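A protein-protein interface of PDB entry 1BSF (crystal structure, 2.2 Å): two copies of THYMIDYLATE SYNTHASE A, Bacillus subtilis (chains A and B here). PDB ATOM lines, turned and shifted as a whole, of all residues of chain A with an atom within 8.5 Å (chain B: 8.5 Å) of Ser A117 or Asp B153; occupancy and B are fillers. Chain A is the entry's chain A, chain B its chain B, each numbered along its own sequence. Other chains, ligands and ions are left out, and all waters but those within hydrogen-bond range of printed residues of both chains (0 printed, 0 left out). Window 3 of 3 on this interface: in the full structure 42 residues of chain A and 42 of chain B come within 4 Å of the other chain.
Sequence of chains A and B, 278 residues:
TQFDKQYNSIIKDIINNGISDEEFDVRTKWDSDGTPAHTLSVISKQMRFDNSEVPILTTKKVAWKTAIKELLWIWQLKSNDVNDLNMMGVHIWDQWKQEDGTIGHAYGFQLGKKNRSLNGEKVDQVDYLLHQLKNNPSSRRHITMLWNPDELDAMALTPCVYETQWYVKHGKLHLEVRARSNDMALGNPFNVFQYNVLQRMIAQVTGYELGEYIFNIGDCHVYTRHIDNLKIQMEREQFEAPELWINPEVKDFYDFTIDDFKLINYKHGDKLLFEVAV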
ATOM      1  N   LYS A 114      -9.711  10.875 -32.469  1.00  0.00           N
ATOM      2  CA  LYS A 114      -9.886  11.423 -31.132  1.00  0.00           C
ATOM      3  C   LYS A 114      -9.093  10.531 -30.189  1.00  0.00           C
ATOM      4  O   LYS A 114      -9.672   9.710 -29.471  1.00  0.00           O
ATOM      5  CB  LYS A 114     -11.361  11.414 -30.738  1.00  0.00           C
ATOM      6  CG  LYS A 114     -12.280  11.982 -31.791  1.00  0.00           C
ATOM      7  CD  LYS A 114     -12.241  13.496 -31.809  1.00  0.00           C
ATOM      8  CE  LYS A 114     -13.150  14.047 -32.910  1.00  0.00           C
ATOM      9  NZ  LYS A 114     -12.501  15.094 -33.772  1.00  0.00           N
ATOM     10  N   ASN A 115      -7.769  10.693 -30.193  1.00  0.00           N
ATOM     11  CA  ASN A 115      -6.905   9.855 -29.362  1.00  0.00           C
ATOM     12  C   ASN A 115      -6.317  10.463 -28.090  1.00  0.00           C
ATOM     13  O   ASN A 115      -5.659   9.761 -27.321  1.00  0.00           O
ATOM     14  CB  ASN A 115      -5.757   9.285 -30.212  1.00  0.00           C
ATOM     15  CG  ASN A 115      -4.999  10.360 -30.983  1.00  0.00           C
ATOM     16  OD1 ASN A 115      -4.606  11.384 -30.424  1.00  0.00           O
ATOM     17  ND2 ASN A 115      -4.790  10.126 -32.273  1.00  0.00           N
ATOM     18  N   ARG A 116      -6.552  11.744 -27.841  1.00  0.00           N
ATOM     19  CA  ARG A 116      -5.972  12.356 -26.648  1.00  0.00           C
ATOM     20  C   ARG A 116      -7.002  12.692 -25.590  1.00  0.00           C
ATOM     21  O   ARG A 116      -8.168  12.938 -25.896  1.00  0.00           O
ATOM     22  CB  ARG A 116      -5.175  13.621 -27.012  1.00  0.00           C
ATOM     23  CG  ARG A 116      -4.294  13.499 -28.253  1.00  0.00           C
ATOM     24  CD  ARG A 116      -3.041  12.663 -28.007  1.00  0.00           C
ATOM     25  NE  ARG A 116      -2.621  12.643 -26.605  1.00  0.00           N
ATOM     26  CZ  ARG A 116      -1.400  12.974 -26.187  1.00  0.00           C
ATOM     27  NH1 ARG A 116      -0.481  13.360 -27.064  1.00  0.00           N
ATOM     28  NH2 ARG A 116      -1.090  12.915 -24.894  1.00  0.00           N
ATOM     29  N   SER A 117      -6.559  12.691 -24.337  1.00  0.00           N
ATOM     30  CA  SER A 117      -7.441  12.998 -23.221  1.00  0.00           C
ATOM     31  C   SER A 117      -7.305  14.467 -22.843  1.00  0.00           C
ATOM     32  O   SER A 117      -6.208  14.949 -22.554  1.00  0.00           O
ATOM     33  CB  SER A 117      -7.106  12.103 -22.031  1.00  0.00           C
ATOM     34  OG  SER A 117      -6.853  10.784 -22.475  1.00  0.00           O
ATOM     35  N   LEU A 118      -8.429  15.177 -22.862  1.00  0.00           N
ATOM     36  CA  LEU A 118      -8.442  16.592 -22.526  1.00  0.00           C
ATOM     37  C   LEU A 118      -9.646  16.933 -21.655  1.00  0.00           C
ATOM     38  O   LEU A 118     -10.748  17.161 -22.148  1.00  0.00           O
ATOM     39  CB  LEU A 118      -8.461  17.430 -23.807  1.00  0.00           C
ATOM     40  CG  LEU A 118      -8.477  18.955 -23.673  1.00  0.00           C
ATOM     41  CD1 LEU A 118      -7.199  19.539 -24.263  1.00  0.00           C
ATOM     42  CD2 LEU A 118      -9.706  19.514 -24.385  1.00  0.00           C
ATOM     43  N   ASN A 119      -9.417  16.954 -20.346  1.00  0.00           N
ATOM     44  CA  ASN A 119     -10.455  17.271 -19.372  1.00  0.00           C
ATOM     45  C   ASN A 119     -11.621  16.297 -19.430  1.00  0.00           C
ATOM     46  O   ASN A 119     -12.751  16.671 -19.733  1.00  0.00           O
ATOM     47  CB  ASN A 119     -10.933  18.712 -19.584  1.00  0.00           C
ATOM     48  CG  ASN A 119      -9.775  19.709 -19.611  1.00  0.00           C
ATOM     49  OD1 ASN A 119      -8.875  19.671 -18.760  1.00  0.00           O
ATOM     50  ND2 ASN A 119      -9.792  20.603 -20.594  1.00  0.00           N
ATOM     51  N   GLY A 120     -11.321  15.037 -19.130  1.00  0.00           N
ATOM     52  CA  GLY A 120     -12.332  13.998 -19.130  1.00  0.00           C
ATOM     53  C   GLY A 120     -13.099  13.903 -20.427  1.00  0.00           C
ATOM     54  O   GLY A 120     -14.287  13.583 -20.425  1.00  0.00           O
ATOM     55  N   GLU A 121     -12.420  14.179 -21.536  1.00  0.00           N
ATOM     56  CA  GLU A 121     -13.049  14.130 -22.857  1.00  0.00           C
ATOM     57  C   GLU A 121     -11.990  13.985 -23.946  1.00  0.00           C
ATOM     58  O   GLU A 121     -11.099  14.824 -24.080  1.00  0.00           O
ATOM     59  CB  GLU A 121     -13.871  15.397 -23.093  1.00  0.00           C
ATOM     60  CG  GLU A 121     -14.996  15.232 -24.099  1.00  0.00           C
ATOM     61  CD  GLU A 121     -15.097  16.416 -25.048  1.00  0.00           C
ATOM     62  OE1 GLU A 121     -14.530  17.481 -24.725  1.00  0.00           O
ATOM     63  OE2 GLU A 121     -15.738  16.287 -26.116  1.00  0.00           O
ATOM     64  N   LYS A 122     -12.096  12.912 -24.723  1.00  0.00           N
ATOM     65  CA  LYS A 122     -11.145  12.637 -25.794  1.00  0.00           C
ATOM     66  C   LYS A 122     -11.144  13.714 -26.883  1.00  0.00           C
ATOM     67  O   LYS A 122     -12.155  14.371 -27.138  1.00  0.00           O
ATOM     68  CB  LYS A 122     -11.445  11.268 -26.412  1.00  0.00           C
ATOM     69  CG  LYS A 122     -11.313  10.106 -25.432  1.00  0.00           C
ATOM     70  CD  LYS A 122     -10.354   9.047 -25.951  1.00  0.00           C
ATOM     71  CE  LYS A 122      -9.451   8.527 -24.845  1.00  0.00           C
ATOM     72  NZ  LYS A 122      -8.016   8.886 -25.082  1.00  0.00           N
ATOM     73  N   VAL A 123      -9.999  13.885 -27.529  1.00  0.00           N
ATOM     74  CA  VAL A 123      -9.864  14.880 -28.577  1.00  0.00           C
ATOM     75  C   VAL A 123      -8.761  14.450 -29.550  1.00  0.00           C
ATOM     76  O   VAL A 123      -7.976  13.556 -29.235  1.00  0.00           O
ATOM     77  CB  VAL A 123      -9.562  16.261 -27.946  1.00  0.00           C
ATOM     78  CG1 VAL A 123      -8.126  16.687 -28.230  1.00  0.00           C
ATOM     79  CG2 VAL A 123     -10.566  17.279 -28.456  1.00  0.00           C
ATOM     80  N   ASP A 124      -8.708  15.078 -30.724  1.00  0.00           N
ATOM     81  CA  ASP A 124      -7.711  14.731 -31.743  1.00  0.00           C
ATOM     82  C   ASP A 124      -6.456  15.610 -31.771  1.00  0.00           C
ATOM     83  O   ASP A 124      -6.437  16.708 -31.218  1.00  0.00           O
ATOM     84  CB  ASP A 124      -8.365  14.750 -33.122  1.00  0.00           C
ATOM     85  CG  ASP A 124      -8.971  16.092 -33.452  1.00  0.00           C
ATOM     86  OD1 ASP A 124      -8.224  17.093 -33.481  1.00  0.00           O
ATOM     87  OD2 ASP A 124     -10.195  16.144 -33.676  1.00  0.00           O
ATOM     88  N   TYR A 128      -5.896  19.100 -29.822  1.00  0.00           N
ATOM     89  CA  TYR A 128      -4.993  19.065 -28.683  1.00  0.00           C
ATOM     90  C   TYR A 128      -3.885  20.088 -28.876  1.00  0.00           C
ATOM     91  O   TYR A 128      -3.565  20.857 -27.969  1.00  0.00           O
ATOM     92  CB  TYR A 128      -4.367  17.686 -28.554  1.00  0.00           C
ATOM     93  CG  TYR A 128      -3.626  17.492 -27.254  1.00  0.00           C
ATOM     94  CD1 TYR A 128      -4.308  17.149 -26.085  1.00  0.00           C
ATOM     95  CD2 TYR A 128      -2.246  17.648 -27.187  1.00  0.00           C
ATOM     96  CE1 TYR A 128      -3.625  16.968 -24.880  1.00  0.00           C
ATOM     97  CE2 TYR A 128      -1.564  17.469 -25.993  1.00  0.00           C
ATOM     98  CZ  TYR A 128      -2.260  17.135 -24.847  1.00  0.00           C
ATOM     99  OH  TYR A 128      -1.589  17.001 -23.661  1.00  0.00           O
ATOM    100  N   GLN A 132      -3.382  23.479 -25.999  1.00  0.00           N
ATOM    101  CA  GLN A 132      -2.104  23.528 -25.294  1.00  0.00           C
ATOM    102  C   GLN A 132      -1.234  24.711 -25.655  1.00  0.00           C
ATOM    103  O   GLN A 132      -0.491  25.211 -24.821  1.00  0.00           O
ATOM    104  CB  GLN A 132      -1.320  22.240 -25.538  1.00  0.00           C
ATOM    105  CG  GLN A 132      -1.914  21.027 -24.843  1.00  0.00           C
ATOM    106  CD  GLN A 132      -2.410  21.342 -23.443  1.00  0.00           C
ATOM    107  OE1 GLN A 132      -3.370  22.096 -23.268  1.00  0.00           O
ATOM    108  NE2 GLN A 132      -1.761  20.764 -22.437  1.00  0.00           N
ATOM    109  N   ARG A 141       6.426  19.828 -26.019  1.00  0.00           N
ATOM    110  CA  ARG A 141       5.785  18.633 -26.583  1.00  0.00           C
ATOM    111  C   ARG A 141       4.814  18.884 -27.748  1.00  0.00           C
ATOM    112  O   ARG A 141       4.246  17.941 -28.304  1.00  0.00           O
ATOM    113  CB  ARG A 141       5.045  17.871 -25.472  1.00  0.00           C
ATOM    114  CG  ARG A 141       5.884  16.827 -24.748  1.00  0.00           C
ATOM    115  CD  ARG A 141       5.808  16.999 -23.233  1.00  0.00           C
ATOM    116  NE  ARG A 141       5.143  15.873 -22.580  1.00  0.00           N
ATOM    117  CZ  ARG A 141       4.044  15.982 -21.836  1.00  0.00           C
ATOM    118  NH1 ARG A 141       3.483  17.170 -21.650  1.00  0.00           N
ATOM    119  NH2 ARG A 141       3.504  14.905 -21.280  1.00  0.00           N
ATOM    120  N   GLN B  98       6.368   2.279 -12.796  1.00  0.00           N
ATOM    121  CA  GLN B  98       4.943   2.238 -12.480  1.00  0.00           C
ATOM    122  C   GLN B  98       4.650   1.072 -11.536  1.00  0.00           C
ATOM    123  O   GLN B  98       5.420   0.123 -11.453  1.00  0.00           O
ATOM    124  CB  GLN B  98       4.120   2.089 -13.769  1.00  0.00           C
ATOM    125  CG  GLN B  98       3.959   3.379 -14.575  1.00  0.00           C
ATOM    126  CD  GLN B  98       2.734   3.362 -15.488  1.00  0.00           C
ATOM    127  OE1 GLN B  98       2.659   4.109 -16.466  1.00  0.00           O
ATOM    128  NE2 GLN B  98       1.767   2.505 -15.164  1.00  0.00           N
ATOM    129  N   ILE B 103       7.349   1.364 -17.584  1.00  0.00           N
ATOM    130  CA  ILE B 103       7.201   2.796 -17.830  1.00  0.00           C
ATOM    131  C   ILE B 103       6.023   3.039 -18.770  1.00  0.00           C
ATOM    132  O   ILE B 103       5.931   4.092 -19.421  1.00  0.00           O
ATOM    133  CB  ILE B 103       8.463   3.374 -18.491  1.00  0.00           C
ATOM    134  CG1 ILE B 103       9.143   2.296 -19.340  1.00  0.00           C
ATOM    135  CG2 ILE B 103       9.414   3.890 -17.429  1.00  0.00           C
ATOM    136  CD1 ILE B 103       9.875   2.829 -20.552  1.00  0.00           C
ATOM    137  N   GLY B 104       5.131   2.058 -18.859  1.00  0.00           N
ATOM    138  CA  GLY B 104       3.974   2.194 -19.723  1.00  0.00           C
ATOM    139  C   GLY B 104       4.249   1.839 -21.175  1.00  0.00           C
ATOM    140  O   GLY B 104       5.159   1.058 -21.475  1.00  0.00           O
ATOM    141  N   HIS B 105       3.460   2.433 -22.074  1.00  0.00           N
ATOM    142  CA  HIS B 105       3.551   2.199 -23.514  1.00  0.00           C
ATOM    143  C   HIS B 105       4.530   3.120 -24.230  1.00  0.00           C
ATOM    144  O   HIS B 105       4.173   3.820 -25.187  1.00  0.00           O
ATOM    145  CB  HIS B 105       2.168   2.350 -24.154  1.00  0.00           C
ATOM    146  CG  HIS B 105       1.202   1.272 -23.771  1.00  0.00           C
ATOM    147  ND1 HIS B 105       0.142   0.904 -24.573  1.00  0.00           N
ATOM    148  CD2 HIS B 105       1.148   0.465 -22.684  1.00  0.00           C
ATOM    149  CE1 HIS B 105      -0.521  -0.083 -23.996  1.00  0.00           C
ATOM    150  NE2 HIS B 105       0.069  -0.368 -22.850  1.00  0.00           N
ATOM    151  N   ASN B 148       4.126   7.598 -30.636  1.00  0.00           N
ATOM    152  CA  ASN B 148       2.858   6.993 -31.034  1.00  0.00           C
ATOM    153  C   ASN B 148       1.721   7.886 -30.563  1.00  0.00           C
ATOM    154  O   ASN B 148       1.442   7.965 -29.363  1.00  0.00           O
ATOM    155  CB  ASN B 148       2.694   5.616 -30.401  1.00  0.00           C
ATOM    156  CG  ASN B 148       1.552   4.846 -30.987  1.00  0.00           C
ATOM    157  OD1 ASN B 148       0.799   5.360 -31.820  1.00  0.00           O
ATOM    158  ND2 ASN B 148       1.406   3.602 -30.563  1.00  0.00           N
ATOM    159  N   PRO B 149       1.037   8.552 -31.506  1.00  0.00           N
ATOM    160  CA  PRO B 149      -0.078   9.448 -31.186  1.00  0.00           C
ATOM    161  C   PRO B 149      -1.210   8.710 -30.499  1.00  0.00           C
ATOM    162  O   PRO B 149      -2.005   9.303 -29.775  1.00  0.00           O
ATOM    163  CB  PRO B 149      -0.498  10.001 -32.541  1.00  0.00           C
ATOM    164  CG  PRO B 149      -0.011   8.986 -33.532  1.00  0.00           C
ATOM    165  CD  PRO B 149       1.271   8.461 -32.954  1.00  0.00           C
ATOM    166  N   ASP B 150      -1.267   7.403 -30.723  1.00  0.00           N
ATOM    167  CA  ASP B 150      -2.307   6.574 -30.138  1.00  0.00           C
ATOM    168  C   ASP B 150      -2.082   6.198 -28.683  1.00  0.00           C
ATOM    169  O   ASP B 150      -3.036   6.117 -27.921  1.00  0.00           O
ATOM    170  CB  ASP B 150      -2.489   5.296 -30.964  1.00  0.00           C
ATOM    171  CG  ASP B 150      -3.271   5.536 -32.237  1.00  0.00           C
ATOM    172  OD1 ASP B 150      -4.042   6.520 -32.288  1.00  0.00           O
ATOM    173  OD2 ASP B 150      -3.109   4.742 -33.188  1.00  0.00           O
ATOM    174  N   GLU B 151      -0.832   5.979 -28.291  1.00  0.00           N
ATOM    175  CA  GLU B 151      -0.550   5.574 -26.914  1.00  0.00           C
ATOM    176  C   GLU B 151       0.270   6.566 -26.097  1.00  0.00           C
ATOM    177  O   GLU B 151       0.862   6.206 -25.074  1.00  0.00           O
ATOM    178  CB  GLU B 151       0.149   4.216 -26.912  1.00  0.00           C
ATOM    179  CG  GLU B 151      -0.281   3.320 -28.060  1.00  0.00           C
ATOM    180  CD  GLU B 151       0.041   1.870 -27.805  1.00  0.00           C
ATOM    181  OE1 GLU B 151       1.166   1.451 -28.139  1.00  0.00           O
ATOM    182  OE2 GLU B 151      -0.824   1.151 -27.269  1.00  0.00           O
ATOM    183  N   LEU B 152       0.296   7.811 -26.552  1.00  0.00           N
ATOM    184  CA  LEU B 152       1.031   8.864 -25.870  1.00  0.00           C
ATOM    185  C   LEU B 152       0.529   9.042 -24.444  1.00  0.00           C
ATOM    186  O   LEU B 152       1.314   9.208 -23.507  1.00  0.00           O
ATOM    187  CB  LEU B 152       0.869  10.174 -26.635  1.00  0.00           C
ATOM    188  CG  LEU B 152       2.023  10.501 -27.580  1.00  0.00           C
ATOM    189  CD1 LEU B 152       1.630  11.643 -28.520  1.00  0.00           C
ATOM    190  CD2 LEU B 152       3.242  10.876 -26.747  1.00  0.00           C
ATOM    191  N   ASP B 153      -0.788   9.015 -24.294  1.00  0.00           N
ATOM    192  CA  ASP B 153      -1.431   9.178 -23.004  1.00  0.00           C
ATOM    193  C   ASP B 153      -1.154   7.973 -22.143  1.00  0.00           C
ATOM    194  O   ASP B 153      -1.393   8.012 -20.941  1.00  0.00           O
ATOM    195  CB  ASP B 153      -2.948   9.311 -23.170  1.00  0.00           C
ATOM    196  CG  ASP B 153      -3.384  10.728 -23.491  1.00  0.00           C
ATOM    197  OD1 ASP B 153      -2.901  11.286 -24.495  1.00  0.00           O
ATOM    198  OD2 ASP B 153      -4.216  11.281 -22.739  1.00  0.00           O
ATOM    199  N   ALA B 154      -0.656   6.900 -22.758  1.00  0.00           N
ATOM    200  CA  ALA B 154      -0.383   5.660 -22.026  1.00  0.00           C
ATOM    201  C   ALA B 154       1.066   5.440 -21.614  1.00  0.00           C
ATOM    202  O   ALA B 154       1.369   4.460 -20.922  1.00  0.00           O
ATOM    203  CB  ALA B 154      -0.863   4.463 -22.836  1.00  0.00           C
ATOM    204  N   MET B 155       1.967   6.320 -22.042  1.00  0.00           N
ATOM    205  CA  MET B 155       3.372   6.175 -21.671  1.00  0.00           C
ATOM    206  C   MET B 155       3.585   6.937 -20.384  1.00  0.00           C
ATOM    207  O   MET B 155       2.956   7.971 -20.163  1.00  0.00           O
ATOM    208  CB  MET B 155       4.288   6.753 -22.742  1.00  0.00           C
ATOM    209  CG  MET B 155       3.683   6.827 -24.103  1.00  0.00           C
ATOM    210  SD  MET B 155       4.924   7.171 -25.345  1.00  0.00           S
ATOM    211  CE  MET B 155       4.083   6.554 -26.803  1.00  0.00           C
ATOM    212  N   ALA B 156       4.476   6.434 -19.536  1.00  0.00           N
ATOM    213  CA  ALA B 156       4.751   7.093 -18.273  1.00  0.00           C
ATOM    214  C   ALA B 156       5.694   8.273 -18.466  1.00  0.00           C
ATOM    215  O   ALA B 156       6.056   8.949 -17.506  1.00  0.00           O
ATOM    216  CB  ALA B 156       5.335   6.107 -17.292  1.00  0.00           C
ATOM    217  N   LEU B 157       6.093   8.513 -19.714  1.00  0.00           N
ATOM    218  CA  LEU B 157       6.981   9.629 -20.061  1.00  0.00           C
ATOM    219  C   LEU B 157       7.187   9.754 -21.567  1.00  0.00           C
ATOM    220  O   LEU B 157       7.363   8.761 -22.271  1.00  0.00           O
ATOM    221  CB  LEU B 157       8.337   9.492 -19.361  1.00  0.00           C
ATOM    222  CG  LEU B 157       8.989   8.116 -19.187  1.00  0.00           C
ATOM    223  CD1 LEU B 157       9.173   7.432 -20.530  1.00  0.00           C
ATOM    224  CD2 LEU B 157      10.332   8.297 -18.514  1.00  0.00           C
ATOM    225  N   THR B 158       7.161  10.991 -22.053  1.00  0.00           N
ATOM    226  CA  THR B 158       7.337  11.286 -23.470  1.00  0.00           C
ATOM    227  C   THR B 158       8.808  11.208 -23.890  1.00  0.00           C
ATOM    228  O   THR B 158       9.648  11.948 -23.381  1.00  0.00           O
ATOM    229  CB  THR B 158       6.819  12.690 -23.787  1.00  0.00           C
ATOM    230  OG1 THR B 158       6.469  13.350 -22.562  1.00  0.00           O
ATOM    231  CG2 THR B 158       5.597  12.615 -24.684  1.00  0.00           C
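The backbone carbonyl oxygen (O) of Pro B149 sits close to the side-chain amide oxygen (OD1) of Asn A115.
The side-chain carboxylate of Asp B153 is in salt-bridge range of the guanidinium group of Arg A116.
The side-chain carboxylate of Asp B153 sits at hydrogen-bond distance from the side-chain hydroxyl of Ser A117, 2.7 Å away.
OG1 of Thr B158 sits at hydrogen-bond distance from NE of Arg A141 (2.9 Å).
The backbone carbonyl oxygen (O) of Asn A115 is in hydrogen-bond range of the side-chain amino group (NZ) of Lys A122 (3.4 Å).
N of Asn A115 sits at hydrogen-bond distance from O of Val A123 (3.0 Å).
The backbone NH (N) of Val A123 sits at hydrogen-bond distance from the backbone carbonyl oxygen (O) of Arg A116 (2.6 Å).
NZ of Lys A122 sits at hydrogen-bond distance from OG of Ser A117 (3.4 Å).
The backbone NH (N) of Asp B150 sits close to the side-chain amide oxygen (OD1) of Asn B148 (3.1 Å).
Asn A115 touches Asp B150 (ND2 to OD1, 3.7 Å).
Arg A116 touches Pro B149 (CD to O, 3.9 Å).
Arg A116 touches Leu B152.
Printed residues of chain B within 4 Å of Asn A115: Pro B149 and Asp B150.
Ser A117 touches just one residue of chain B: Asp B153 (2.7 Å).
Gly A120 touches none of the printed residues of chain B.
Glu A121 touches none of the printed residues of chain B.
Printed residues of chain A within 4 Å of Pro B149: Asn A115 (3.4 Å) and Arg A116 (3.9 Å).
Printed residues of chain A within 4 Å of Leu B152: Arg A116 (3.1 Å).
Asp B153 touches just these residues of chain A: Arg A116 (2.5 Å) and Ser A117 (2.7 Å).
Of the printed residues of chain A, Thr B158 touches Arg A141.
The nearest residue of chain B that does not touch Ser A117 is Ala B154 (7.3 Å).
The nearest residue of chain A that does not touch Asp B153 is Asn A115 (4.2 Å).
The nearest printed residue of chain A that does not touch Pro B149 is Lys A114 (7.2 Å).
Printed residues of chain A that touch a printed residue of chain B: Asn A115, Arg A116, Ser A117 and Arg A141.
Among the printed residues, 7 pairs touch across the chains.
No position is printed for both chains.
Of the 7 pairs that touch across the chains among the printed residues, none has its exchanged pair printed and touching as well.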
